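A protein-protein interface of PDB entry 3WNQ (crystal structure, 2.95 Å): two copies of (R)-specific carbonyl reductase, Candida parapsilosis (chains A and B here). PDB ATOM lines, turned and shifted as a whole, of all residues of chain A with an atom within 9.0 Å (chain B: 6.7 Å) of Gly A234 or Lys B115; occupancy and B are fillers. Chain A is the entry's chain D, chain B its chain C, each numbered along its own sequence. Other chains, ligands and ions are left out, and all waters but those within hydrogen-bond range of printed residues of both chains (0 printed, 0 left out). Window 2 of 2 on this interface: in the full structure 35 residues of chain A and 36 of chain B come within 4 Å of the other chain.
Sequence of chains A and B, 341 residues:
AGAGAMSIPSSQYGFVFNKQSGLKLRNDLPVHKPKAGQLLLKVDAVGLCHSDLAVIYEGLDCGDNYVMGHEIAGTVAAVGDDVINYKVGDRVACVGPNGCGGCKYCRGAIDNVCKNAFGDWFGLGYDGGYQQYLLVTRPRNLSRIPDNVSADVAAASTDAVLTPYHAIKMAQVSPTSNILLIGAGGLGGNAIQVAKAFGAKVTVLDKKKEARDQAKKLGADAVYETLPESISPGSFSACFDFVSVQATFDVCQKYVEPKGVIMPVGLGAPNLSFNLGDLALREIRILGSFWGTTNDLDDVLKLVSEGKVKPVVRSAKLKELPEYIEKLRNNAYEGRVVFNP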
ATOM      1  N   ASN A 178      19.756  -7.023 -25.901  1.00  0.00           N
ATOM      2  CA  ASN A 178      21.018  -7.721 -25.962  1.00  0.00           C
ATOM      3  C   ASN A 178      21.126  -8.395 -24.618  1.00  0.00           C
ATOM      4  O   ASN A 178      21.587  -7.828 -23.651  1.00  0.00           O
ATOM      5  CB  ASN A 178      22.193  -6.758 -26.206  1.00  0.00           C
ATOM      6  CG  ASN A 178      23.582  -7.446 -26.052  1.00  0.00           C
ATOM      7  OD1 ASN A 178      23.856  -8.545 -26.642  1.00  0.00           O
ATOM      8  ND2 ASN A 178      24.470  -6.792 -25.258  1.00  0.00           N
ATOM      9  N   LEU A 227      33.019 -15.575 -20.345  1.00  0.00           N
ATOM     10  CA  LEU A 227      32.861 -14.367 -21.115  1.00  0.00           C
ATOM     11  C   LEU A 227      34.245 -13.805 -21.418  1.00  0.00           C
ATOM     12  O   LEU A 227      35.068 -13.618 -20.527  1.00  0.00           O
ATOM     13  CB  LEU A 227      32.000 -13.373 -20.341  1.00  0.00           C
ATOM     14  CG  LEU A 227      30.764 -12.978 -21.127  1.00  0.00           C
ATOM     15  CD1 LEU A 227      30.123 -14.166 -21.748  1.00  0.00           C
ATOM     16  CD2 LEU A 227      29.819 -12.327 -20.193  1.00  0.00           C
ATOM     17  N   ILE A 231      34.273  -8.740 -24.700  1.00  0.00           N
ATOM     18  CA  ILE A 231      32.897  -8.419 -24.302  1.00  0.00           C
ATOM     19  C   ILE A 231      33.037  -7.434 -23.158  1.00  0.00           C
ATOM     20  O   ILE A 231      33.563  -7.756 -22.072  1.00  0.00           O
ATOM     21  CB  ILE A 231      32.108  -9.638 -23.810  1.00  0.00           C
ATOM     22  CG1 ILE A 231      31.745 -10.549 -24.984  1.00  0.00           C
ATOM     23  CG2 ILE A 231      30.836  -9.182 -23.139  1.00  0.00           C
ATOM     24  CD1 ILE A 231      30.616 -10.048 -25.866  1.00  0.00           C
ATOM     25  N   SER A 232      32.561  -6.229 -23.450  1.00  0.00           N
ATOM     26  CA  SER A 232      32.610  -5.080 -22.577  1.00  0.00           C
ATOM     27  C   SER A 232      31.645  -5.139 -21.373  1.00  0.00           C
ATOM     28  O   SER A 232      30.518  -5.555 -21.507  1.00  0.00           O
ATOM     29  CB  SER A 232      32.330  -3.876 -23.465  1.00  0.00           C
ATOM     30  OG  SER A 232      32.497  -2.697 -22.758  1.00  0.00           O
ATOM     31  N   PRO A 233      32.089  -4.739 -20.176  1.00  0.00           N
ATOM     32  CA  PRO A 233      31.213  -4.765 -19.001  1.00  0.00           C
ATOM     33  C   PRO A 233      30.034  -3.811 -19.116  1.00  0.00           C
ATOM     34  O   PRO A 233      30.059  -2.880 -19.928  1.00  0.00           O
ATOM     35  CB  PRO A 233      32.136  -4.360 -17.867  1.00  0.00           C
ATOM     36  CG  PRO A 233      33.413  -4.925 -18.290  1.00  0.00           C
ATOM     37  CD  PRO A 233      33.482  -4.560 -19.756  1.00  0.00           C
ATOM     38  N   GLY A 234      29.007  -4.048 -18.302  1.00  0.00           N
ATOM     39  CA  GLY A 234      27.819  -3.209 -18.296  1.00  0.00           C
ATOM     40  C   GLY A 234      27.320  -2.914 -19.678  1.00  0.00           C
ATOM     41  O   GLY A 234      27.108  -1.754 -20.003  1.00  0.00           O
ATOM     42  N   SER A 235      27.113  -3.962 -20.472  1.00  0.00           N
ATOM     43  CA  SER A 235      26.639  -3.825 -21.840  1.00  0.00           C
ATOM     44  C   SER A 235      25.392  -4.676 -22.195  1.00  0.00           C
ATOM     45  O   SER A 235      24.896  -4.637 -23.340  1.00  0.00           O
ATOM     46  CB  SER A 235      27.770  -4.196 -22.780  1.00  0.00           C
ATOM     47  OG  SER A 235      28.033  -5.602 -22.711  1.00  0.00           O
ATOM     48  N   PHE A 236      24.887  -5.462 -21.254  1.00  0.00           N
ATOM     49  CA  PHE A 236      23.716  -6.275 -21.554  1.00  0.00           C
ATOM     50  C   PHE A 236      22.494  -5.630 -20.942  1.00  0.00           C
ATOM     51  O   PHE A 236      22.556  -5.158 -19.810  1.00  0.00           O
ATOM     52  CB  PHE A 236      23.884  -7.683 -20.998  1.00  0.00           C
ATOM     53  CG  PHE A 236      24.908  -8.501 -21.735  1.00  0.00           C
ATOM     54  CD1 PHE A 236      24.564  -9.167 -22.903  1.00  0.00           C
ATOM     55  CD2 PHE A 236      26.248  -8.528 -21.320  1.00  0.00           C
ATOM     56  CE1 PHE A 236      25.523  -9.838 -23.652  1.00  0.00           C
ATOM     57  CE2 PHE A 236      27.204  -9.197 -22.073  1.00  0.00           C
ATOM     58  CZ  PHE A 236      26.833  -9.849 -23.240  1.00  0.00           C
ATOM     59  N   SER A 237      21.392  -5.601 -21.705  1.00  0.00           N
ATOM     60  CA  SER A 237      20.128  -5.017 -21.279  1.00  0.00           C
ATOM     61  C   SER A 237      19.477  -5.860 -20.193  1.00  0.00           C
ATOM     62  O   SER A 237      18.805  -5.347 -19.296  1.00  0.00           O
ATOM     63  CB  SER A 237      19.198  -4.858 -22.496  1.00  0.00           C
ATOM     64  OG  SER A 237      19.079  -6.028 -23.291  1.00  0.00           O
ATOM     65  N   ALA A 238      19.702  -7.162 -20.265  1.00  0.00           N
ATOM     66  CA  ALA A 238      19.155  -8.059 -19.269  1.00  0.00           C
ATOM     67  C   ALA A 238      19.989  -9.317 -19.116  1.00  0.00           C
ATOM     68  O   ALA A 238      20.506  -9.862 -20.089  1.00  0.00           O
ATOM     69  CB  ALA A 238      17.760  -8.425 -19.639  1.00  0.00           C
ATOM     70  N   CYS A 239      20.104  -9.773 -17.879  1.00  0.00           N
ATOM     71  CA  CYS A 239      20.850 -10.972 -17.548  1.00  0.00           C
ATOM     72  C   CYS A 239      19.968 -11.970 -16.847  1.00  0.00           C
ATOM     73  O   CYS A 239      19.355 -11.662 -15.826  1.00  0.00           O
ATOM     74  CB  CYS A 239      22.000 -10.635 -16.614  1.00  0.00           C
ATOM     75  SG  CYS A 239      23.190  -9.648 -17.430  1.00  0.00           S
ATOM     76  N   ASP A 250      27.286 -12.452  -9.657  1.00  0.00           N
ATOM     77  CA  ASP A 250      28.324 -11.448  -9.776  1.00  0.00           C
ATOM     78  C   ASP A 250      28.668 -11.107 -11.209  1.00  0.00           C
ATOM     79  O   ASP A 250      29.032  -9.969 -11.555  1.00  0.00           O
ATOM     80  CB  ASP A 250      29.561 -11.911  -9.056  1.00  0.00           C
ATOM     81  CG  ASP A 250      29.485 -11.645  -7.592  1.00  0.00           C
ATOM     82  OD1 ASP A 250      28.494 -11.025  -7.134  1.00  0.00           O
ATOM     83  OD2 ASP A 250      30.412 -12.041  -6.881  1.00  0.00           O
ATOM     84  N   VAL A 251      28.555 -12.106 -12.056  1.00  0.00           N
ATOM     85  CA  VAL A 251      28.834 -11.917 -13.460  1.00  0.00           C
ATOM     86  C   VAL A 251      27.758 -11.027 -14.094  1.00  0.00           C
ATOM     87  O   VAL A 251      28.046 -10.151 -14.944  1.00  0.00           O
ATOM     88  CB  VAL A 251      28.829 -13.246 -14.125  1.00  0.00           C
ATOM     89  CG1 VAL A 251      29.196 -13.093 -15.622  1.00  0.00           C
ATOM     90  CG2 VAL A 251      29.759 -14.130 -13.380  1.00  0.00           C
ATOM     91  N   CYS A 252      26.516 -11.283 -13.674  1.00  0.00           N
ATOM     92  CA  CYS A 252      25.384 -10.515 -14.141  1.00  0.00           C
ATOM     93  C   CYS A 252      25.546  -9.063 -13.746  1.00  0.00           C
ATOM     94  O   CYS A 252      25.451  -8.197 -14.586  1.00  0.00           O
ATOM     95  CB  CYS A 252      24.097 -11.049 -13.540  1.00  0.00           C
ATOM     96  SG  CYS A 252      23.627 -12.697 -14.109  1.00  0.00           S
ATOM     97  N   GLN A 253      25.805  -8.804 -12.470  1.00  0.00           N
ATOM     98  CA  GLN A 253      25.928  -7.445 -12.022  1.00  0.00           C
ATOM     99  C   GLN A 253      27.113  -6.744 -12.650  1.00  0.00           C
ATOM    100  O   GLN A 253      27.160  -5.499 -12.726  1.00  0.00           O
ATOM    101  CB  GLN A 253      26.038  -7.389 -10.515  1.00  0.00           C
ATOM    102  CG  GLN A 253      26.111  -5.976 -10.031  1.00  0.00           C
ATOM    103  CD  GLN A 253      25.981  -5.847  -8.541  1.00  0.00           C
ATOM    104  OE1 GLN A 253      26.052  -6.851  -7.806  1.00  0.00           O
ATOM    105  NE2 GLN A 253      25.793  -4.603  -8.066  1.00  0.00           N
ATOM    106  N   LYS A 254      28.075  -7.529 -13.123  1.00  0.00           N
ATOM    107  CA  LYS A 254      29.257  -6.949 -13.733  1.00  0.00           C
ATOM    108  C   LYS A 254      28.987  -6.556 -15.177  1.00  0.00           C
ATOM    109  O   LYS A 254      29.391  -5.493 -15.655  1.00  0.00           O
ATOM    110  CB  LYS A 254      30.395  -7.963 -13.676  1.00  0.00           C
ATOM    111  CG  LYS A 254      31.614  -7.498 -14.440  1.00  0.00           C
ATOM    112  CD  LYS A 254      32.677  -8.555 -14.596  1.00  0.00           C
ATOM    113  CE  LYS A 254      33.895  -7.957 -15.244  1.00  0.00           C
ATOM    114  NZ  LYS A 254      34.956  -8.986 -15.309  1.00  0.00           N
ATOM    115  N   TYR A 255      28.277  -7.445 -15.858  1.00  0.00           N
ATOM    116  CA  TYR A 255      27.954  -7.289 -17.274  1.00  0.00           C
ATOM    117  C   TYR A 255      26.619  -6.637 -17.694  1.00  0.00           C
ATOM    118  O   TYR A 255      26.425  -6.317 -18.873  1.00  0.00           O
ATOM    119  CB  TYR A 255      28.126  -8.660 -17.966  1.00  0.00           C
ATOM    120  CG  TYR A 255      29.592  -9.018 -18.158  1.00  0.00           C
ATOM    121  CD1 TYR A 255      30.363  -8.335 -19.098  1.00  0.00           C
ATOM    122  CD2 TYR A 255      30.230 -10.002 -17.358  1.00  0.00           C
ATOM    123  CE1 TYR A 255      31.724  -8.615 -19.249  1.00  0.00           C
ATOM    124  CE2 TYR A 255      31.616 -10.285 -17.500  1.00  0.00           C
ATOM    125  CZ  TYR A 255      32.339  -9.588 -18.449  1.00  0.00           C
ATOM    126  OH  TYR A 255      33.656  -9.855 -18.669  1.00  0.00           O
ATOM    127  N   VAL A 256      25.716  -6.432 -16.745  1.00  0.00           N
ATOM    128  CA  VAL A 256      24.431  -5.811 -17.041  1.00  0.00           C
ATOM    129  C   VAL A 256      24.700  -4.332 -17.169  1.00  0.00           C
ATOM    130  O   VAL A 256      25.541  -3.806 -16.436  1.00  0.00           O
ATOM    131  CB  VAL A 256      23.451  -6.032 -15.911  1.00  0.00           C
ATOM    132  CG1 VAL A 256      23.937  -5.361 -14.681  1.00  0.00           C
ATOM    133  CG2 VAL A 256      22.133  -5.512 -16.283  1.00  0.00           C
ATOM    134  N   GLU A 257      24.001  -3.657 -18.094  1.00  0.00           N
ATOM    135  CA  GLU A 257      24.212  -2.229 -18.307  1.00  0.00           C
ATOM    136  C   GLU A 257      23.432  -1.369 -17.326  1.00  0.00           C
ATOM    137  O   GLU A 257      22.630  -1.845 -16.533  1.00  0.00           O
ATOM    138  CB  GLU A 257      23.843  -1.843 -19.741  1.00  0.00           C
ATOM    139  CG  GLU A 257      22.395  -1.572 -19.960  1.00  0.00           C
ATOM    140  CD  GLU A 257      21.985  -1.602 -21.428  1.00  0.00           C
ATOM    141  OE1 GLU A 257      20.772  -1.547 -21.715  1.00  0.00           O
ATOM    142  OE2 GLU A 257      22.860  -1.686 -22.306  1.00  0.00           O
ATOM    143  N   PRO A 258      23.716  -0.072 -17.326  1.00  0.00           N
ATOM    144  CA  PRO A 258      22.975   0.778 -16.405  1.00  0.00           C
ATOM    145  C   PRO A 258      21.463   0.641 -16.690  1.00  0.00           C
ATOM    146  O   PRO A 258      21.022   0.493 -17.841  1.00  0.00           O
ATOM    147  CB  PRO A 258      23.535   2.161 -16.720  1.00  0.00           C
ATOM    148  CG  PRO A 258      24.966   1.878 -17.057  1.00  0.00           C
ATOM    149  CD  PRO A 258      24.864   0.649 -17.921  1.00  0.00           C
ATOM    150  N   LYS A 259      20.680   0.695 -15.622  1.00  0.00           N
ATOM    151  CA  LYS A 259      19.227   0.576 -15.653  1.00  0.00           C
ATOM    152  C   LYS A 259      18.800  -0.809 -16.179  1.00  0.00           C
ATOM    153  O   LYS A 259      17.622  -1.047 -16.449  1.00  0.00           O
ATOM    154  CB  LYS A 259      18.602   1.715 -16.476  1.00  0.00           C
ATOM    155  CG  LYS A 259      17.166   2.012 -16.106  1.00  0.00           C
ATOM    156  CD  LYS A 259      17.079   2.775 -14.858  1.00  0.00           C
ATOM    157  CE  LYS A 259      15.725   2.583 -14.252  1.00  0.00           C
ATOM    158  NZ  LYS A 259      15.420   3.615 -13.223  1.00  0.00           N
ATOM    159  N   GLY A 260      19.762  -1.733 -16.277  1.00  0.00           N
ATOM    160  CA  GLY A 260      19.497  -3.088 -16.744  1.00  0.00           C
ATOM    161  C   GLY A 260      18.738  -3.961 -15.766  1.00  0.00           C
ATOM    162  O   GLY A 260      18.378  -3.525 -14.680  1.00  0.00           O
ATOM    163  N   ASP A 278      27.191  -0.293  -6.533  1.00  0.00           N
ATOM    164  CA  ASP A 278      27.030  -0.460  -7.972  1.00  0.00           C
ATOM    165  C   ASP A 278      25.548  -0.450  -8.391  1.00  0.00           C
ATOM    166  O   ASP A 278      25.158   0.271  -9.348  1.00  0.00           O
ATOM    167  CB  ASP A 278      27.667  -1.764  -8.484  1.00  0.00           C
ATOM    168  CG  ASP A 278      27.463  -1.958 -10.002  1.00  0.00           C
ATOM    169  OD1 ASP A 278      28.028  -1.167 -10.782  1.00  0.00           O
ATOM    170  OD2 ASP A 278      26.723  -2.872 -10.436  1.00  0.00           O
ATOM    171  N   LEU A 281      24.233   3.183  -7.918  1.00  0.00           N
ATOM    172  CA  LEU A 281      24.813   4.139  -8.846  1.00  0.00           C
ATOM    173  C   LEU A 281      24.444   3.923 -10.325  1.00  0.00           C
ATOM    174  O   LEU A 281      24.417   4.874 -11.128  1.00  0.00           O
ATOM    175  CB  LEU A 281      26.334   4.151  -8.686  1.00  0.00           C
ATOM    176  CG  LEU A 281      26.978   5.032  -9.764  1.00  0.00           C
ATOM    177  CD1 LEU A 281      26.989   6.461  -9.360  1.00  0.00           C
ATOM    178  CD2 LEU A 281      28.358   4.603  -9.997  1.00  0.00           C
ATOM    179  N   ARG A 282      24.162   2.680 -10.690  1.00  0.00           N
ATOM    180  CA  ARG A 282      23.815   2.384 -12.072  1.00  0.00           C
ATOM    181  C   ARG A 282      22.335   1.966 -12.289  1.00  0.00           C
ATOM    182  O   ARG A 282      21.977   1.431 -13.352  1.00  0.00           O
ATOM    183  CB  ARG A 282      24.782   1.319 -12.615  1.00  0.00           C
ATOM    184  CG  ARG A 282      26.248   1.722 -12.600  1.00  0.00           C
ATOM    185  CD  ARG A 282      27.092   0.814 -13.464  1.00  0.00           C
ATOM    186  NE  ARG A 282      26.848  -0.570 -13.129  1.00  0.00           N
ATOM    187  CZ  ARG A 282      26.639  -1.515 -14.041  1.00  0.00           C
ATOM    188  NH1 ARG A 282      26.404  -2.773 -13.674  1.00  0.00           N
ATOM    189  NH2 ARG A 282      26.676  -1.197 -15.341  1.00  0.00           N
ATOM    190  N   ILE A 284      20.562  -0.406 -11.447  1.00  0.00           N
ATOM    191  CA  ILE A 284      20.326  -1.824 -11.747  1.00  0.00           C
ATOM    192  C   ILE A 284      19.052  -2.323 -11.034  1.00  0.00           C
ATOM    193  O   ILE A 284      18.809  -1.978  -9.888  1.00  0.00           O
ATOM    194  CB  ILE A 284      21.507  -2.715 -11.262  1.00  0.00           C
ATOM    195  CG1 ILE A 284      22.531  -2.867 -12.352  1.00  0.00           C
ATOM    196  CG2 ILE A 284      21.038  -4.077 -10.973  1.00  0.00           C
ATOM    197  CD1 ILE A 284      23.067  -1.621 -12.762  1.00  0.00           C
ATOM    198  N   CYS B 100      25.752  14.006 -20.221  1.00  0.00           N
ATOM    199  CA  CYS B 100      26.322  14.469 -21.496  1.00  0.00           C
ATOM    200  C   CYS B 100      25.319  14.998 -22.559  1.00  0.00           C
ATOM    201  O   CYS B 100      25.721  15.651 -23.531  1.00  0.00           O
ATOM    202  CB  CYS B 100      27.140  13.337 -22.115  1.00  0.00           C
ATOM    203  SG  CYS B 100      26.239  12.275 -23.243  1.00  0.00           S
ATOM    204  N   CYS B 103      24.069  10.852 -25.451  1.00  0.00           N
ATOM    205  CA  CYS B 103      24.153   9.391 -25.551  1.00  0.00           C
ATOM    206  C   CYS B 103      22.795   8.708 -25.369  1.00  0.00           C
ATOM    207  O   CYS B 103      21.804   9.355 -25.013  1.00  0.00           O
ATOM    208  CB  CYS B 103      25.108   8.859 -24.502  1.00  0.00           C
ATOM    209  SG  CYS B 103      24.462   8.958 -22.832  1.00  0.00           S
ATOM    210  N   LYS B 104      22.753   7.389 -25.570  1.00  0.00           N
ATOM    211  CA  LYS B 104      21.498   6.659 -25.427  1.00  0.00           C
ATOM    212  C   LYS B 104      20.805   6.845 -24.065  1.00  0.00           C
ATOM    213  O   LYS B 104      19.577   6.872 -23.988  1.00  0.00           O
ATOM    214  CB  LYS B 104      21.709   5.159 -25.766  1.00  0.00           C
ATOM    215  CG  LYS B 104      22.074   4.134 -24.643  1.00  0.00           C
ATOM    216  CD  LYS B 104      22.147   2.706 -25.253  1.00  0.00           C
ATOM    217  CE  LYS B 104      22.210   1.588 -24.254  1.00  0.00           C
ATOM    218  NZ  LYS B 104      20.978   0.727 -24.226  1.00  0.00           N
ATOM    219  N   TYR B 105      21.574   7.006 -22.992  1.00  0.00           N
ATOM    220  CA  TYR B 105      20.950   7.183 -21.684  1.00  0.00           C
ATOM    221  C   TYR B 105      20.332   8.587 -21.517  1.00  0.00           C
ATOM    222  O   TYR B 105      19.213   8.693 -21.020  1.00  0.00           O
ATOM    223  CB  TYR B 105      21.959   6.892 -20.542  1.00  0.00           C
ATOM    224  CG  TYR B 105      22.568   5.501 -20.583  1.00  0.00           C
ATOM    225  CD1 TYR B 105      21.984   4.409 -19.907  1.00  0.00           C
ATOM    226  CD2 TYR B 105      23.668   5.241 -21.392  1.00  0.00           C
ATOM    227  CE1 TYR B 105      22.483   3.060 -20.063  1.00  0.00           C
ATOM    228  CE2 TYR B 105      24.177   3.908 -21.555  1.00  0.00           C
ATOM    229  CZ  TYR B 105      23.577   2.824 -20.904  1.00  0.00           C
ATOM    230  OH  TYR B 105      24.029   1.547 -21.193  1.00  0.00           O
ATOM    231  N   CYS B 106      21.034   9.647 -21.946  1.00  0.00           N
ATOM    232  CA  CYS B 106      20.515  11.016 -21.788  1.00  0.00           C
ATOM    233  C   CYS B 106      19.298  11.296 -22.658  1.00  0.00           C
ATOM    234  O   CYS B 106      18.310  11.922 -22.226  1.00  0.00           O
ATOM    235  CB  CYS B 106      21.594  12.050 -22.119  1.00  0.00           C
ATOM    236  SG  CYS B 106      23.043  12.010 -21.057  1.00  0.00           S
ATOM    237  N   ASP B 111      19.552  10.706 -17.753  1.00  0.00           N
ATOM    238  CA  ASP B 111      20.838  11.357 -17.803  1.00  0.00           C
ATOM    239  C   ASP B 111      21.630  11.183 -16.490  1.00  0.00           C
ATOM    240  O   ASP B 111      22.849  11.495 -16.409  1.00  0.00           O
ATOM    241  CB  ASP B 111      20.645  12.839 -18.139  1.00  0.00           C
ATOM    242  CG  ASP B 111      19.530  13.487 -17.357  1.00  0.00           C
ATOM    243  OD1 ASP B 111      19.588  13.602 -16.090  1.00  0.00           O
ATOM    244  OD2 ASP B 111      18.589  13.890 -18.068  1.00  0.00           O
ATOM    245  N   VAL B 113      22.492   8.480 -15.255  1.00  0.00           N
ATOM    246  CA  VAL B 113      23.387   7.340 -15.295  1.00  0.00           C
ATOM    247  C   VAL B 113      24.341   7.348 -16.485  1.00  0.00           C
ATOM    248  O   VAL B 113      25.012   6.332 -16.751  1.00  0.00           O
ATOM    249  CB  VAL B 113      22.618   6.050 -15.282  1.00  0.00           C
ATOM    250  CG1 VAL B 113      21.922   5.910 -13.951  1.00  0.00           C
ATOM    251  CG2 VAL B 113      21.639   6.041 -16.454  1.00  0.00           C
ATOM    252  N   CYS B 114      24.413   8.514 -17.150  1.00  0.00           N
ATOM    253  CA  CYS B 114      25.245   8.787 -18.327  1.00  0.00           C
ATOM    254  C   CYS B 114      26.639   8.268 -18.102  1.00  0.00           C
ATOM    255  O   CYS B 114      27.328   8.713 -17.187  1.00  0.00           O
ATOM    256  CB  CYS B 114      25.299  10.297 -18.591  1.00  0.00           C
ATOM    257  SG  CYS B 114      26.170  10.852 -20.050  1.00  0.00           S
ATOM    258  N   LYS B 115      27.061   7.319 -18.939  1.00  0.00           N
ATOM    259  CA  LYS B 115      28.400   6.760 -18.797  1.00  0.00           C
ATOM    260  C   LYS B 115      29.441   7.837 -19.119  1.00  0.00           C
ATOM    261  O   LYS B 115      30.474   7.930 -18.463  1.00  0.00           O
ATOM    262  CB  LYS B 115      28.579   5.558 -19.717  1.00  0.00           C
ATOM    263  CG  LYS B 115      27.936   4.258 -19.227  1.00  0.00           C
ATOM    264  CD  LYS B 115      28.264   3.116 -20.213  1.00  0.00           C
ATOM    265  CE  LYS B 115      27.452   1.821 -20.015  1.00  0.00           C
ATOM    266  NZ  LYS B 115      27.191   1.109 -21.344  1.00  0.00           N
ATOM    267  N   ASN B 116      29.139   8.676 -20.110  1.00  0.00           N
ATOM    268  CA  ASN B 116      30.023   9.740 -20.559  1.00  0.00           C
ATOM    269  C   ASN B 116      30.311  10.821 -19.574  1.00  0.00           C
ATOM    270  O   ASN B 116      31.332  11.487 -19.667  1.00  0.00           O
ATOM    271  CB  ASN B 116      29.448  10.406 -21.797  1.00  0.00           C
ATOM    272  CG  ASN B 116      29.450   9.489 -23.008  1.00  0.00           C
ATOM    273  OD1 ASN B 116      29.900   8.351 -22.931  1.00  0.00           O
ATOM    274  ND2 ASN B 116      28.953   9.979 -24.130  1.00  0.00           N
ATOM    275  N   ALA B 117      29.407  11.027 -18.632  1.00  0.00           N
ATOM    276  CA  ALA B 117      29.590  12.111 -17.666  1.00  0.00           C
ATOM    277  C   ALA B 117      30.251  11.718 -16.379  1.00  0.00           C
ATOM    278  O   ALA B 117      30.335  12.521 -15.476  1.00  0.00           O
ATOM    279  CB  ALA B 117      28.235  12.807 -17.395  1.00  0.00           C
ATOM    280  N   PHE B 118      30.735  10.488 -16.307  1.00  0.00           N
ATOM    281  CA  PHE B 118      31.410   9.992 -15.114  1.00  0.00           C
ATOM    282  C   PHE B 118      32.655  10.817 -14.686  1.00  0.00           C
ATOM    283  O   PHE B 118      33.629  10.969 -15.442  1.00  0.00           O
ATOM    284  CB  PHE B 118      31.793   8.558 -15.348  1.00  0.00           C
ATOM    285  CG  PHE B 118      31.239   7.638 -14.348  1.00  0.00           C
ATOM    286  CD1 PHE B 118      31.570   7.794 -13.010  1.00  0.00           C
ATOM    287  CD2 PHE B 118      30.428   6.584 -14.744  1.00  0.00           C
ATOM    288  CE1 PHE B 118      31.103   6.902 -12.076  1.00  0.00           C
ATOM    289  CE2 PHE B 118      29.947   5.670 -13.834  1.00  0.00           C
ATOM    290  CZ  PHE B 118      30.278   5.816 -12.498  1.00  0.00           C
ATOM    291  N   GLY B 119      32.622  11.348 -13.459  1.00  0.00           N
ATOM    292  CA  GLY B 119      33.726  12.175 -13.031  1.00  0.00           C
ATOM    293  C   GLY B 119      33.666  13.552 -13.710  1.00  0.00           C
ATOM    294  O   GLY B 119      34.681  14.243 -13.811  1.00  0.00           O
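SG of Cys B103 sits close to N of Tyr B105 (3.5 Å).
NZ of Lys B115 lies within hydrogen-bond range of OH of Tyr B105 (3.2 Å).
N of Gly A234 lies within hydrogen-bond range of O of Lys A254 (3.0 Å).
The backbone NH of Gly A234 sits close to the backbone carbonyl oxygen of Tyr A255.
The backbone carbonyl oxygen of Phe A236 is in hydrogen-bond range of the backbone NH of Glu A257, 2.7 Å away.
Hydrophobic or aromatic side chains of chain A that line the printed part of chain B: Pro A258 and Leu A281.
Among the printed residues, 7 pairs touch across the chains.
NZ of Lys B104 lies within salt-bridge range of OE1 of Glu A257 (3.4 Å).
The side-chain amino group (NZ) of Lys B115 sits at hydrogen-bond distance from the backbone carbonyl oxygen (O) of Gly A234 (3.2 Å).
No position is printed for both chains.
Of the 7 pairs that touch across the chains among the printed residues, none has its exchanged pair printed and touching as well.
OH of Tyr B105 touches OE2 of Glu A257 (3.6 Å).
Pro A258 touches Tyr B105.
Pro A258 touches Lys B115 (CD to CE, 3.5 Å).
Leu A281 touches Val B113.
CZ of Phe B118 touches CD2 of Leu A281, 3.4 Å away.
Of chain B, only Lys B115 (3.2 Å) comes within 4 Å of Gly A234.
Of the printed residues of chain A, Lys B115 touches Gly A234 and Pro A258.
No residue of chain A comes within 4 Å of Cys B114.
Printed residues of chain B within 4 Å of Leu A281: Val B113 (3.9 Å) and Phe B118 (3.4 Å).
Of the printed residues of chain A, Phe B118 touches Leu A281.
Lys A254 touches none of the printed residues of chain B.
Ala B117 touches none of the printed residues of chain A.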
